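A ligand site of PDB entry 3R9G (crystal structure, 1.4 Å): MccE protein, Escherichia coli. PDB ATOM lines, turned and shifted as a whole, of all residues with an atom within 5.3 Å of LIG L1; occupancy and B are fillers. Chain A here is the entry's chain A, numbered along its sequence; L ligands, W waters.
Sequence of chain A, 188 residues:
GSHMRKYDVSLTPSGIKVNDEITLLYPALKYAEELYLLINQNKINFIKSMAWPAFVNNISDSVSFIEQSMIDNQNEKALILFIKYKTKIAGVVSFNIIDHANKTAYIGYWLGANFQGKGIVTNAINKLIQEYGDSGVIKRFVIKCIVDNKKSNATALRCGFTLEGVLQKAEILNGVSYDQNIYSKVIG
The indole nitrogen (NE1) of Trp 52 is in hydrogen-bond range of an oxygen (O2) of LIG L1, at 2.9 Å. N1 of LIG L1 sits at hydrogen-bond distance from O of Lys 144 (2.8 Å). An oxygen (O9) of LIG L1 sits close to the side-chain amide oxygen (OE1) of Gln 180, 3.3 Å away. O4 of LIG L1 sits close to N of Tyr 109, 3.4 Å away. The side-chain hydroxyl of Ser 152 sits close to a sulfur (S1) of LG2 L2 (3.3 Å). N3 of LIG L1 sits at hydrogen-bond distance from NE1 of Trp 110 (3.1 Å). The side-chain amide nitrogen (ND2) of Asn 96 sits at hydrogen-bond distance from an oxygen (O1) of LIG L1. OG of Ser 94 is in hydrogen-bond range of O4 of LIG L1, at 2.8 Å. The backbone carbonyl oxygen (O) of Tyr 109 lies within hydrogen-bond range of a nitrogen (N7) of LG2 L2, at 2.9 Å. The backbone carbonyl oxygen (O) of Gly 108 lies close to an oxygen (O4) of LIG L1 (3.3 Å).
SD of Met 50 sits close to O2 of LIG L1 (3.7 Å). O of Ile 107 lies close to O6 of LIG L1, at 3.1 Å. Ile 39 touches LIG L1 (CD1 to N2, 3.8 Å). Phe 65 touches LIG L1. CD1 of Ile 80 touches O3 of LIG L1 (3.9 Å). Val 92 touches LIG L1. Ile 143 touches LIG L1. Glu 171 touches LIG L1 (OE1 to C8, 3.6 Å). Hydrophobic or aromatic side chains within 4 Å of LIG L1: Ile 39, Met 50, Trp 52, Phe 65, Ile 80, Val 92, Tyr 109, Trp 110 and Ile 143. Of the 22 residues printed, 16 come within 4 Å of LIG L1.
Water W1 bridges O10 of LIG L1 and ND2 of Asn 96. Water W5 bridges an oxygen (O2) of LIG L1 and the backbone NH of Ala 51. Water W3 lies within hydrogen-bond range of OE2 of Glu 171 (2.6 Å) and N6 of LIG L1 (2.8 Å).
A sulfur (S1) of LG2 L2 sits close to a nitrogen (N1) of LIG L1 (3.5 Å).
The side-chain hydroxyl (OH) of Tyr 109 lies within hydrogen-bond range of the side-chain hydroxyl (OG) of Ser 152, 2.9 Å away. The side-chain amide oxygen of Gln 180 sits close to the side-chain carboxylate of Glu 171, 2.8 Å away. N of Trp 110 is in hydrogen-bond range of O of Val 92 (3.0 Å). O of Gly 108 sits at hydrogen-bond distance from N of Ser 94 (2.9 Å). The indole nitrogen (NE1) of Trp 52 sits at hydrogen-bond distance from the side-chain sulfur (SD) of Met 50 (3.7 Å). OD1 of Asn 96 is in hydrogen-bond range of OG of Ser 94.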
ATOM      1  N   LEU A  35     -11.752  -3.384  23.981  1.00  0.00           N
ATOM      2  CA  LEU A  35     -10.975  -2.191  23.670  1.00  0.00           C
ATOM      3  C   LEU A  35     -11.861  -1.149  23.000  1.00  0.00           C
ATOM      4  O   LEU A  35     -11.858   0.036  23.392  1.00  0.00           O
ATOM      5  CB  LEU A  35      -9.782  -2.533  22.767  1.00  0.00           C
ATOM      6  CG  LEU A  35      -8.827  -1.365  22.435  1.00  0.00           C
ATOM      7  CD1 LEU A  35      -8.055  -0.895  23.678  1.00  0.00           C
ATOM      8  CD2 LEU A  35      -7.840  -1.750  21.329  1.00  0.00           C
ATOM      9  N   ILE A  39     -12.822   2.657  24.414  1.00  0.00           N
ATOM     10  CA  ILE A  39     -12.570   3.870  23.652  1.00  0.00           C
ATOM     11  C   ILE A  39     -13.864   4.659  23.459  1.00  0.00           C
ATOM     12  O   ILE A  39     -13.914   5.854  23.682  1.00  0.00           O
ATOM     13  CB  ILE A  39     -11.908   3.579  22.290  1.00  0.00           C
ATOM     14  CG1 ILE A  39     -10.499   3.026  22.490  1.00  0.00           C
ATOM     15  CG2 ILE A  39     -11.870   4.840  21.409  1.00  0.00           C
ATOM     16  CD1 ILE A  39      -9.961   2.242  21.306  1.00  0.00           C
ATOM     17  N   MET A  50      -5.838  13.537  22.339  1.00  0.00           N
ATOM     18  CA  MET A  50      -5.319  12.643  21.306  1.00  0.00           C
ATOM     19  C   MET A  50      -6.106  12.802  20.007  1.00  0.00           C
ATOM     20  O   MET A  50      -7.271  13.206  20.039  1.00  0.00           O
ATOM     21  CB  MET A  50      -5.376  11.175  21.790  1.00  0.00           C
ATOM     22  CG  MET A  50      -4.587  10.910  23.075  1.00  0.00           C
ATOM     23  SD  MET A  50      -4.646   9.200  23.653  1.00  0.00           S
ATOM     24  CE  MET A  50      -6.375   9.067  24.133  1.00  0.00           C
ATOM     25  N   ALA A  51      -5.463  12.500  18.875  1.00  0.00           N
ATOM     26  CA  ALA A  51      -6.031  12.784  17.549  1.00  0.00           C
ATOM     27  C   ALA A  51      -6.809  11.642  16.910  1.00  0.00           C
ATOM     28  O   ALA A  51      -7.613  11.880  16.010  1.00  0.00           O
ATOM     29  CB  ALA A  51      -4.917  13.224  16.603  1.00  0.00           C
ATOM     30  N   TRP A  52      -6.520  10.427  17.338  1.00  0.00           N
ATOM     31  CA  TRP A  52      -7.120   9.216  16.778  1.00  0.00           C
ATOM     32  C   TRP A  52      -8.500   8.831  17.320  1.00  0.00           C
ATOM     33  O   TRP A  52      -9.271   8.205  16.593  1.00  0.00           O
ATOM     34  CB  TRP A  52      -6.130   8.019  16.869  1.00  0.00           C
ATOM     35  CG  TRP A  52      -5.706   7.745  18.290  1.00  0.00           C
ATOM     36  CD1 TRP A  52      -4.603   8.236  18.931  1.00  0.00           C
ATOM     37  CD2 TRP A  52      -6.437   6.972  19.259  1.00  0.00           C
ATOM     38  NE1 TRP A  52      -4.585   7.801  20.235  1.00  0.00           N
ATOM     39  CE2 TRP A  52      -5.692   7.023  20.467  1.00  0.00           C
ATOM     40  CE3 TRP A  52      -7.622   6.229  19.219  1.00  0.00           C
ATOM     41  CZ2 TRP A  52      -6.118   6.361  21.619  1.00  0.00           C
ATOM     42  CZ3 TRP A  52      -8.040   5.577  20.366  1.00  0.00           C
ATOM     43  CH2 TRP A  52      -7.288   5.641  21.555  1.00  0.00           C
ATOM     44  N   VAL A  56     -12.530   6.525  15.760  1.00  0.00           N
ATOM     45  CA  VAL A  56     -12.841   5.145  16.179  1.00  0.00           C
ATOM     46  C   VAL A  56     -14.360   4.987  16.261  1.00  0.00           C
ATOM     47  O   VAL A  56     -14.977   5.312  17.274  1.00  0.00           O
ATOM     48  CB  VAL A  56     -12.184   4.778  17.535  1.00  0.00           C
ATOM     49  CG1 VAL A  56     -12.511   3.331  17.911  1.00  0.00           C
ATOM     50  CG2 VAL A  56     -10.671   4.969  17.467  1.00  0.00           C
ATOM     51  N   PHE A  65      -6.517  -1.678  14.267  1.00  0.00           N
ATOM     52  CA  PHE A  65      -5.466  -1.231  15.169  1.00  0.00           C
ATOM     53  C   PHE A  65      -4.705  -2.406  15.788  1.00  0.00           C
ATOM     54  O   PHE A  65      -3.473  -2.390  15.854  1.00  0.00           O
ATOM     55  CB  PHE A  65      -6.037  -0.334  16.277  1.00  0.00           C
ATOM     56  CG  PHE A  65      -5.030   0.036  17.316  1.00  0.00           C
ATOM     57  CD1 PHE A  65      -3.996   0.920  17.009  1.00  0.00           C
ATOM     58  CD2 PHE A  65      -5.107  -0.488  18.606  1.00  0.00           C
ATOM     59  CE1 PHE A  65      -3.058   1.272  17.967  1.00  0.00           C
ATOM     60  CE2 PHE A  65      -4.149  -0.132  19.564  1.00  0.00           C
ATOM     61  CZ  PHE A  65      -3.132   0.736  19.240  1.00  0.00           C
ATOM     62  N   ILE A  80       3.346  -2.245  21.522  1.00  0.00           N
ATOM     63  CA  ILE A  80       2.001  -1.857  21.935  1.00  0.00           C
ATOM     64  C   ILE A  80       1.467  -2.893  22.906  1.00  0.00           C
ATOM     65  O   ILE A  80       1.435  -4.084  22.586  1.00  0.00           O
ATOM     66  CB  ILE A  80       1.051  -1.755  20.710  1.00  0.00           C
ATOM     67  CG1 ILE A  80       1.662  -0.950  19.551  1.00  0.00           C
ATOM     68  CG2 ILE A  80      -0.322  -1.231  21.117  1.00  0.00           C
ATOM     69  CD1 ILE A  80       2.053   0.488  19.856  1.00  0.00           C
ATOM     70  N   VAL A  92      -3.991   1.596  27.235  1.00  0.00           N
ATOM     71  CA  VAL A  92      -2.889   1.147  26.400  1.00  0.00           C
ATOM     72  C   VAL A  92      -1.609   1.826  26.885  1.00  0.00           C
ATOM     73  O   VAL A  92      -1.633   2.991  27.274  1.00  0.00           O
ATOM     74  CB  VAL A  92      -3.144   1.493  24.908  1.00  0.00           C
ATOM     75  CG1 VAL A  92      -1.964   1.114  24.026  1.00  0.00           C
ATOM     76  CG2 VAL A  92      -4.411   0.802  24.420  1.00  0.00           C
ATOM     77  N   VAL A  93      -0.501   1.099  26.896  1.00  0.00           N
ATOM     78  CA  VAL A  93       0.813   1.710  27.083  1.00  0.00           C
ATOM     79  C   VAL A  93       1.715   1.192  25.968  1.00  0.00           C
ATOM     80  O   VAL A  93       1.602   0.045  25.538  1.00  0.00           O
ATOM     81  CB  VAL A  93       1.411   1.429  28.496  1.00  0.00           C
ATOM     82  CG1 VAL A  93       1.636  -0.071  28.715  1.00  0.00           C
ATOM     83  CG2 VAL A  93       2.689   2.222  28.730  1.00  0.00           C
ATOM     84  N   SER A  94       2.591   2.049  25.466  1.00  0.00           N
ATOM     85  CA  SER A  94       3.382   1.673  24.305  1.00  0.00           C
ATOM     86  C   SER A  94       4.784   2.257  24.295  1.00  0.00           C
ATOM     87  O   SER A  94       5.039   3.309  24.887  1.00  0.00           O
ATOM     88  CB  SER A  94       2.674   2.142  23.045  1.00  0.00           C
ATOM     89  OG  SER A  94       2.460   3.541  23.094  1.00  0.00           O
ATOM     90  N   ASN A  96       5.826   3.800  21.269  1.00  0.00           N
ATOM     91  CA  ASN A  96       5.288   4.185  19.941  1.00  0.00           C
ATOM     92  C   ASN A  96       6.314   3.908  18.856  1.00  0.00           C
ATOM     93  O   ASN A  96       5.960   3.496  17.736  1.00  0.00           O
ATOM     94  CB  ASN A  96       4.972   5.681  19.891  1.00  0.00           C
ATOM     95  CG  ASN A  96       3.839   6.083  20.811  1.00  0.00           C
ATOM     96  OD1 ASN A  96       2.890   5.335  21.020  1.00  0.00           O
ATOM     97  ND2 ASN A  96       3.916   7.304  21.345  1.00  0.00           N
ATOM     98  N   ILE A 107       7.557   6.771  24.433  1.00  0.00           N
ATOM     99  CA  ILE A 107       6.445   6.166  25.185  1.00  0.00           C
ATOM    100  C   ILE A 107       5.115   6.882  24.950  1.00  0.00           C
ATOM    101  O   ILE A 107       5.058   8.112  24.877  1.00  0.00           O
ATOM    102  CB  ILE A 107       6.781   6.170  26.704  1.00  0.00           C
ATOM    103  CG1 ILE A 107       7.912   5.182  27.014  1.00  0.00           C
ATOM    104  CG2 ILE A 107       5.538   5.860  27.539  1.00  0.00           C
ATOM    105  CD1 ILE A 107       8.588   5.422  28.344  1.00  0.00           C
ATOM    106  N   GLY A 108       4.052   6.089  24.816  1.00  0.00           N
ATOM    107  CA  GLY A 108       2.688   6.621  24.754  1.00  0.00           C
ATOM    108  C   GLY A 108       1.781   5.916  25.751  1.00  0.00           C
ATOM    109  O   GLY A 108       2.092   4.794  26.183  1.00  0.00           O
ATOM    110  N   TYR A 109       0.665   6.533  26.108  1.00  0.00           N
ATOM    111  CA  TYR A 109      -0.269   5.909  27.052  1.00  0.00           C
ATOM    112  C   TYR A 109      -1.627   6.562  27.080  1.00  0.00           C
ATOM    113  O   TYR A 109      -1.757   7.746  26.776  1.00  0.00           O
ATOM    114  CB  TYR A 109       0.306   5.891  28.484  1.00  0.00           C
ATOM    115  CG  TYR A 109       1.017   7.158  28.928  1.00  0.00           C
ATOM    116  CD1 TYR A 109       0.313   8.306  29.299  1.00  0.00           C
ATOM    117  CD2 TYR A 109       2.408   7.192  28.991  1.00  0.00           C
ATOM    118  CE1 TYR A 109       0.987   9.452  29.719  1.00  0.00           C
ATOM    119  CE2 TYR A 109       3.085   8.324  29.409  1.00  0.00           C
ATOM    120  CZ  TYR A 109       2.374   9.457  29.777  1.00  0.00           C
ATOM    121  OH  TYR A 109       3.054  10.575  30.191  1.00  0.00           O
ATOM    122  N   TRP A 110      -2.631   5.778  27.472  1.00  0.00           N
ATOM    123  CA  TRP A 110      -3.934   6.310  27.870  1.00  0.00           C
ATOM    124  C   TRP A 110      -4.644   5.341  28.812  1.00  0.00           C
ATOM    125  O   TRP A 110      -4.398   4.137  28.774  1.00  0.00           O
ATOM    126  CB  TRP A 110      -4.826   6.633  26.667  1.00  0.00           C
ATOM    127  CG  TRP A 110      -5.267   5.493  25.797  1.00  0.00           C
ATOM    128  CD1 TRP A 110      -4.724   5.135  24.593  1.00  0.00           C
ATOM    129  CD2 TRP A 110      -6.420   4.641  25.987  1.00  0.00           C
ATOM    130  NE1 TRP A 110      -5.440   4.090  24.044  1.00  0.00           N
ATOM    131  CE2 TRP A 110      -6.488   3.775  24.883  1.00  0.00           C
ATOM    132  CE3 TRP A 110      -7.383   4.510  27.005  1.00  0.00           C
ATOM    133  CZ2 TRP A 110      -7.481   2.789  24.749  1.00  0.00           C
ATOM    134  CZ3 TRP A 110      -8.369   3.540  26.874  1.00  0.00           C
ATOM    135  CH2 TRP A 110      -8.412   2.700  25.746  1.00  0.00           C
ATOM    136  N   ILE A 143       9.319  10.686  26.845  1.00  0.00           N
ATOM    137  CA  ILE A 143       7.900  11.039  26.842  1.00  0.00           C
ATOM    138  C   ILE A 143       7.727  12.432  26.280  1.00  0.00           C
ATOM    139  O   ILE A 143       8.361  13.379  26.762  1.00  0.00           O
ATOM    140  CB  ILE A 143       7.273  10.958  28.254  1.00  0.00           C
ATOM    141  CG1 ILE A 143       7.243   9.507  28.755  1.00  0.00           C
ATOM    142  CG2 ILE A 143       5.852  11.568  28.255  1.00  0.00           C
ATOM    143  CD1 ILE A 143       6.956   9.362  30.241  1.00  0.00           C
ATOM    144  N   LYS A 144       6.893  12.567  25.252  1.00  0.00           N
ATOM    145  CA  LYS A 144       6.497  13.857  24.714  1.00  0.00           C
ATOM    146  C   LYS A 144       5.042  14.088  25.034  1.00  0.00           C
ATOM    147  O   LYS A 144       4.207  13.227  24.782  1.00  0.00           O
ATOM    148  CB  LYS A 144       6.660  13.910  23.200  1.00  0.00           C
ATOM    149  CG  LYS A 144       8.052  13.640  22.694  1.00  0.00           C
ATOM    150  CD  LYS A 144       8.066  13.671  21.174  1.00  0.00           C
ATOM    151  CE  LYS A 144       9.455  13.467  20.602  1.00  0.00           C
ATOM    152  NZ  LYS A 144       9.442  13.532  19.105  1.00  0.00           N
ATOM    153  N   CYS A 145       4.718  15.272  25.563  1.00  0.00           N
ATOM    154  CA  CYS A 145       3.320  15.569  25.836  1.00  0.00           C
ATOM    155  C   CYS A 145       3.017  17.057  25.769  1.00  0.00           C
ATOM    156  O   CYS A 145       3.826  17.891  26.155  1.00  0.00           O
ATOM    157  CB  CYS A 145       2.879  14.981  27.178  1.00  0.00           C
ATOM    158  SG  CYS A 145       3.888  15.489  28.571  1.00  0.00           S
ATOM    159  N   SER A 152      -0.709  14.157  32.003  1.00  0.00           N
ATOM    160  CA  SER A 152       0.393  13.460  31.326  1.00  0.00           C
ATOM    161  C   SER A 152       1.758  13.976  31.795  1.00  0.00           C
ATOM    162  O   SER A 152       2.675  13.184  32.024  1.00  0.00           O
ATOM    163  CB  SER A 152       0.280  13.516  29.810  1.00  0.00           C
ATOM    164  OG  SER A 152       1.327  12.737  29.248  1.00  0.00           O
ATOM    165  N   GLU A 171       2.729  19.062  18.045  1.00  0.00           N
ATOM    166  CA  GLU A 171       1.643  18.087  18.011  1.00  0.00           C
ATOM    167  C   GLU A 171       0.355  18.745  17.545  1.00  0.00           C
ATOM    168  O   GLU A 171      -0.072  19.737  18.110  1.00  0.00           O
ATOM    169  CB  GLU A 171       1.440  17.431  19.379  1.00  0.00           C
ATOM    170  CG  GLU A 171       0.481  16.231  19.314  1.00  0.00           C
ATOM    171  CD  GLU A 171       0.364  15.454  20.603  1.00  0.00           C
ATOM    172  OE1 GLU A 171       1.165  15.680  21.541  1.00  0.00           O
ATOM    173  OE2 GLU A 171      -0.544  14.600  20.658  1.00  0.00           O
ATOM    174  N   GLN A 180       4.916  20.800  22.826  1.00  0.00           N
ATOM    175  CA  GLN A 180       5.126  19.623  23.685  1.00  0.00           C
ATOM    176  C   GLN A 180       6.298  19.831  24.611  1.00  0.00           C
ATOM    177  O   GLN A 180       7.330  20.372  24.210  1.00  0.00           O
ATOM    178  CB  GLN A 180       5.423  18.367  22.853  1.00  0.00           C
ATOM    179  CG  GLN A 180       4.261  17.809  22.056  1.00  0.00           C
ATOM    180  CD  GLN A 180       4.693  16.596  21.249  1.00  0.00           C
ATOM    181  OE1 GLN A 180       3.941  15.627  21.101  1.00  0.00           O
ATOM    182  NE2 GLN A 180       5.909  16.639  20.736  1.00  0.00           N
HETATM  183  C1  LIG L   1       1.214  10.092  22.273  1.00  0.00           C
HETATM  184  N1  LIG L   1       2.593  10.984  24.150  1.00  0.00           N
HETATM  185  O1  LIG L   1       1.858   9.038  22.192  1.00  0.00           O
HETATM  186  P1  LIG L   1      -0.851   9.056  20.923  1.00  0.00           P
HETATM  187  N2  LIG L   1      -6.644   2.489  19.553  1.00  0.00           N
HETATM  188  C2  LIG L   1      -6.162   2.331  20.801  1.00  0.00           C
HETATM  189  N3  LIG L   1      -5.029   2.928  21.224  1.00  0.00           N
HETATM  190  C3  LIG L   1      -4.354   3.720  20.356  1.00  0.00           C
HETATM  191  C4  LIG L   1      -4.811   3.909  19.056  1.00  0.00           C
HETATM  192  C5  LIG L   1      -5.996   3.267  18.654  1.00  0.00           C
HETATM  193  N4  LIG L   1      -6.488   3.424  17.406  1.00  0.00           N
HETATM  194  N5  LIG L   1      -3.926   4.726  18.437  1.00  0.00           N
HETATM  195  C6  LIG L   1      -2.957   5.029  19.312  1.00  0.00           C
HETATM  196  N6  LIG L   1       0.002  10.281  21.793  1.00  0.00           N
HETATM  197  N7  LIG L   1      -3.207   4.400  20.478  1.00  0.00           N
HETATM  198  C7  LIG L   1       1.743  11.298  22.994  1.00  0.00           C
HETATM  199  C8  LIG L   1       2.398  12.341  22.071  1.00  0.00           C
HETATM  200  C9  LIG L   1       3.538  11.903  21.186  1.00  0.00           C
HETATM  201  C10 LIG L   1      -2.402   4.457  21.714  1.00  0.00           C
HETATM  202  O2  LIG L   1      -2.328   9.493  20.752  1.00  0.00           O
HETATM  203  C11 LIG L   1      -0.906   4.429  21.485  1.00  0.00           C
HETATM  204  O3  LIG L   1      -0.438   3.089  21.301  1.00  0.00           O
HETATM  205  C12 LIG L   1      -0.366   5.084  22.748  1.00  0.00           C
HETATM  206  O4  LIG L   1      -0.156   4.156  23.818  1.00  0.00           O
HETATM  207  O5  LIG L   1      -0.148   8.813  19.512  1.00  0.00           O
HETATM  208  C13 LIG L   1       0.916   7.904  19.299  1.00  0.00           C
HETATM  209  C14 LIG L   1       1.523   8.226  17.945  1.00  0.00           C
HETATM  210  C15 LIG L   1       2.413   9.466  18.035  1.00  0.00           C
HETATM  211  N8  LIG L   1       2.500  10.092  16.731  1.00  0.00           N
HETATM  212  C16 LIG L   1       2.189  10.166  25.154  1.00  0.00           C
HETATM  213  C17 LIG L   1       1.030   9.540  25.044  1.00  0.00           C
HETATM  214  O6  LIG L   1       2.888   9.942  26.162  1.00  0.00           O
HETATM  215  C18 LIG L   1      -1.493   6.006  23.184  1.00  0.00           C
HETATM  216  O7  LIG L   1      -2.597   5.715  22.332  1.00  0.00           O
HETATM  217  C19 LIG L   1      -1.184   7.492  23.018  1.00  0.00           C
HETATM  218  O8  LIG L   1      -0.701   7.673  21.691  1.00  0.00           O
HETATM  219  O9  LIG L   1       3.671  12.502  20.084  1.00  0.00           O
HETATM  220  O10 LIG L   1       4.330  11.024  21.561  1.00  0.00           O
HETATM  221  N1  LG2 L   2       1.100   4.900  42.436  1.00  0.00           N
HETATM  222  C1  LG2 L   2       1.070   6.097  41.993  1.00  0.00           C
HETATM  223  N2  LG2 L   2       0.016   6.814  41.913  1.00  0.00           N
HETATM  224  C2  LG2 L   2      -1.149   6.368  42.498  1.00  0.00           C
HETATM  225  C3  LG2 L   2      -1.184   5.139  43.060  1.00  0.00           C
HETATM  226  C4  LG2 L   2       0.016   4.312  42.966  1.00  0.00           C
HETATM  227  N3  LG2 L   2      -0.056   3.017  43.256  1.00  0.00           N
HETATM  228  N4  LG2 L   2      -2.431   4.952  43.530  1.00  0.00           N
HETATM  229  C5  LG2 L   2      -3.105   6.103  43.271  1.00  0.00           C
HETATM  230  N5  LG2 L   2      -2.307   6.993  42.642  1.00  0.00           N
HETATM  231  C6  LG2 L   2      -2.786   8.289  42.102  1.00  0.00           C
HETATM  232  C7  LG2 L   2      -1.901   9.502  42.173  1.00  0.00           C
HETATM  233  O1  LG2 L   2      -2.154  10.240  43.364  1.00  0.00           O
HETATM  234  C8  LG2 L   2      -2.334  10.274  40.935  1.00  0.00           C
HETATM  235  O2  LG2 L   2      -3.643  10.833  41.137  1.00  0.00           O
HETATM  236  P1  LG2 L   2      -3.937  12.422  41.054  1.00  0.00           P
HETATM  237  O3  LG2 L   2      -5.276  12.584  41.731  1.00  0.00           O
HETATM  238  O4  LG2 L   2      -3.909  12.789  39.597  1.00  0.00           O
HETATM  239  O5  LG2 L   2      -2.793  13.071  41.792  1.00  0.00           O
HETATM  240  C9  LG2 L   2      -2.539   9.178  39.912  1.00  0.00           C
HETATM  241  O6  LG2 L   2      -2.905   8.020  40.684  1.00  0.00           O
HETATM  242  C10 LG2 L   2      -1.278   8.899  39.085  1.00  0.00           C
HETATM  243  O7  LG2 L   2      -1.494   7.759  38.256  1.00  0.00           O
HETATM  244  P2  LG2 L   2      -0.709   7.564  36.873  1.00  0.00           P
HETATM  245  O8  LG2 L   2       0.481   8.481  36.826  1.00  0.00           O
HETATM  246  O9  LG2 L   2      -0.482   6.101  36.688  1.00  0.00           O
HETATM  247  O10 LG2 L   2      -1.740   8.016  35.724  1.00  0.00           O
HETATM  248  P3  LG2 L   2      -3.190   8.718  35.817  1.00  0.00           P
HETATM  249  O11 LG2 L   2      -4.155   7.743  36.407  1.00  0.00           O
HETATM  250  O12 LG2 L   2      -3.078  10.066  36.441  1.00  0.00           O
HETATM  251  O13 LG2 L   2      -3.521   8.840  34.266  1.00  0.00           O
HETATM  252  C11 LG2 L   2      -3.127   9.658  31.998  1.00  0.00           C
HETATM  253  C12 LG2 L   2      -2.763   9.773  33.474  1.00  0.00           C
HETATM  254  C13 LG2 L   2      -2.320  10.704  31.235  1.00  0.00           C
HETATM  255  C14 LG2 L   2      -2.748   8.249  31.536  1.00  0.00           C
HETATM  256  C15 LG2 L   2      -4.634   9.892  31.880  1.00  0.00           C
HETATM  257  O14 LG2 L   2      -4.939  11.185  32.402  1.00  0.00           O
HETATM  258  C16 LG2 L   2      -5.162   9.774  30.468  1.00  0.00           C
HETATM  259  O15 LG2 L   2      -5.316   8.682  29.950  1.00  0.00           O
HETATM  260  N6  LG2 L   2      -5.452  10.895  29.825  1.00  0.00           N
HETATM  261  C17 LG2 L   2      -6.009  11.025  28.466  1.00  0.00           C
HETATM  262  C18 LG2 L   2      -5.048  10.468  27.420  1.00  0.00           C
HETATM  263  C19 LG2 L   2      -3.738  11.199  27.459  1.00  0.00           C
HETATM  264  O16 LG2 L   2      -3.695  12.390  27.756  1.00  0.00           O
HETATM  265  N7  LG2 L   2      -2.636  10.502  27.187  1.00  0.00           N
HETATM  266  C20 LG2 L   2      -1.269  11.005  27.175  1.00  0.00           C
HETATM  267  C21 LG2 L   2      -1.137  11.908  25.963  1.00  0.00           C
HETATM  268  S1  LG2 L   2       0.398  12.837  26.120  1.00  0.00           S
HETATM  269  O   HOH W   1       6.081   9.298  20.620  1.00  0.00           O
HETATM  270  O   HOH W   2      -8.945   1.114  18.388  1.00  0.00           O
HETATM  271  O   HOH W   3      -1.338  12.693  22.304  1.00  0.00           O
HETATM  272  O   HOH W   4      -8.731   2.264  15.850  1.00  0.00           O
HETATM  273  O   HOH W   5      -2.818  11.443  18.961  1.00  0.00           O
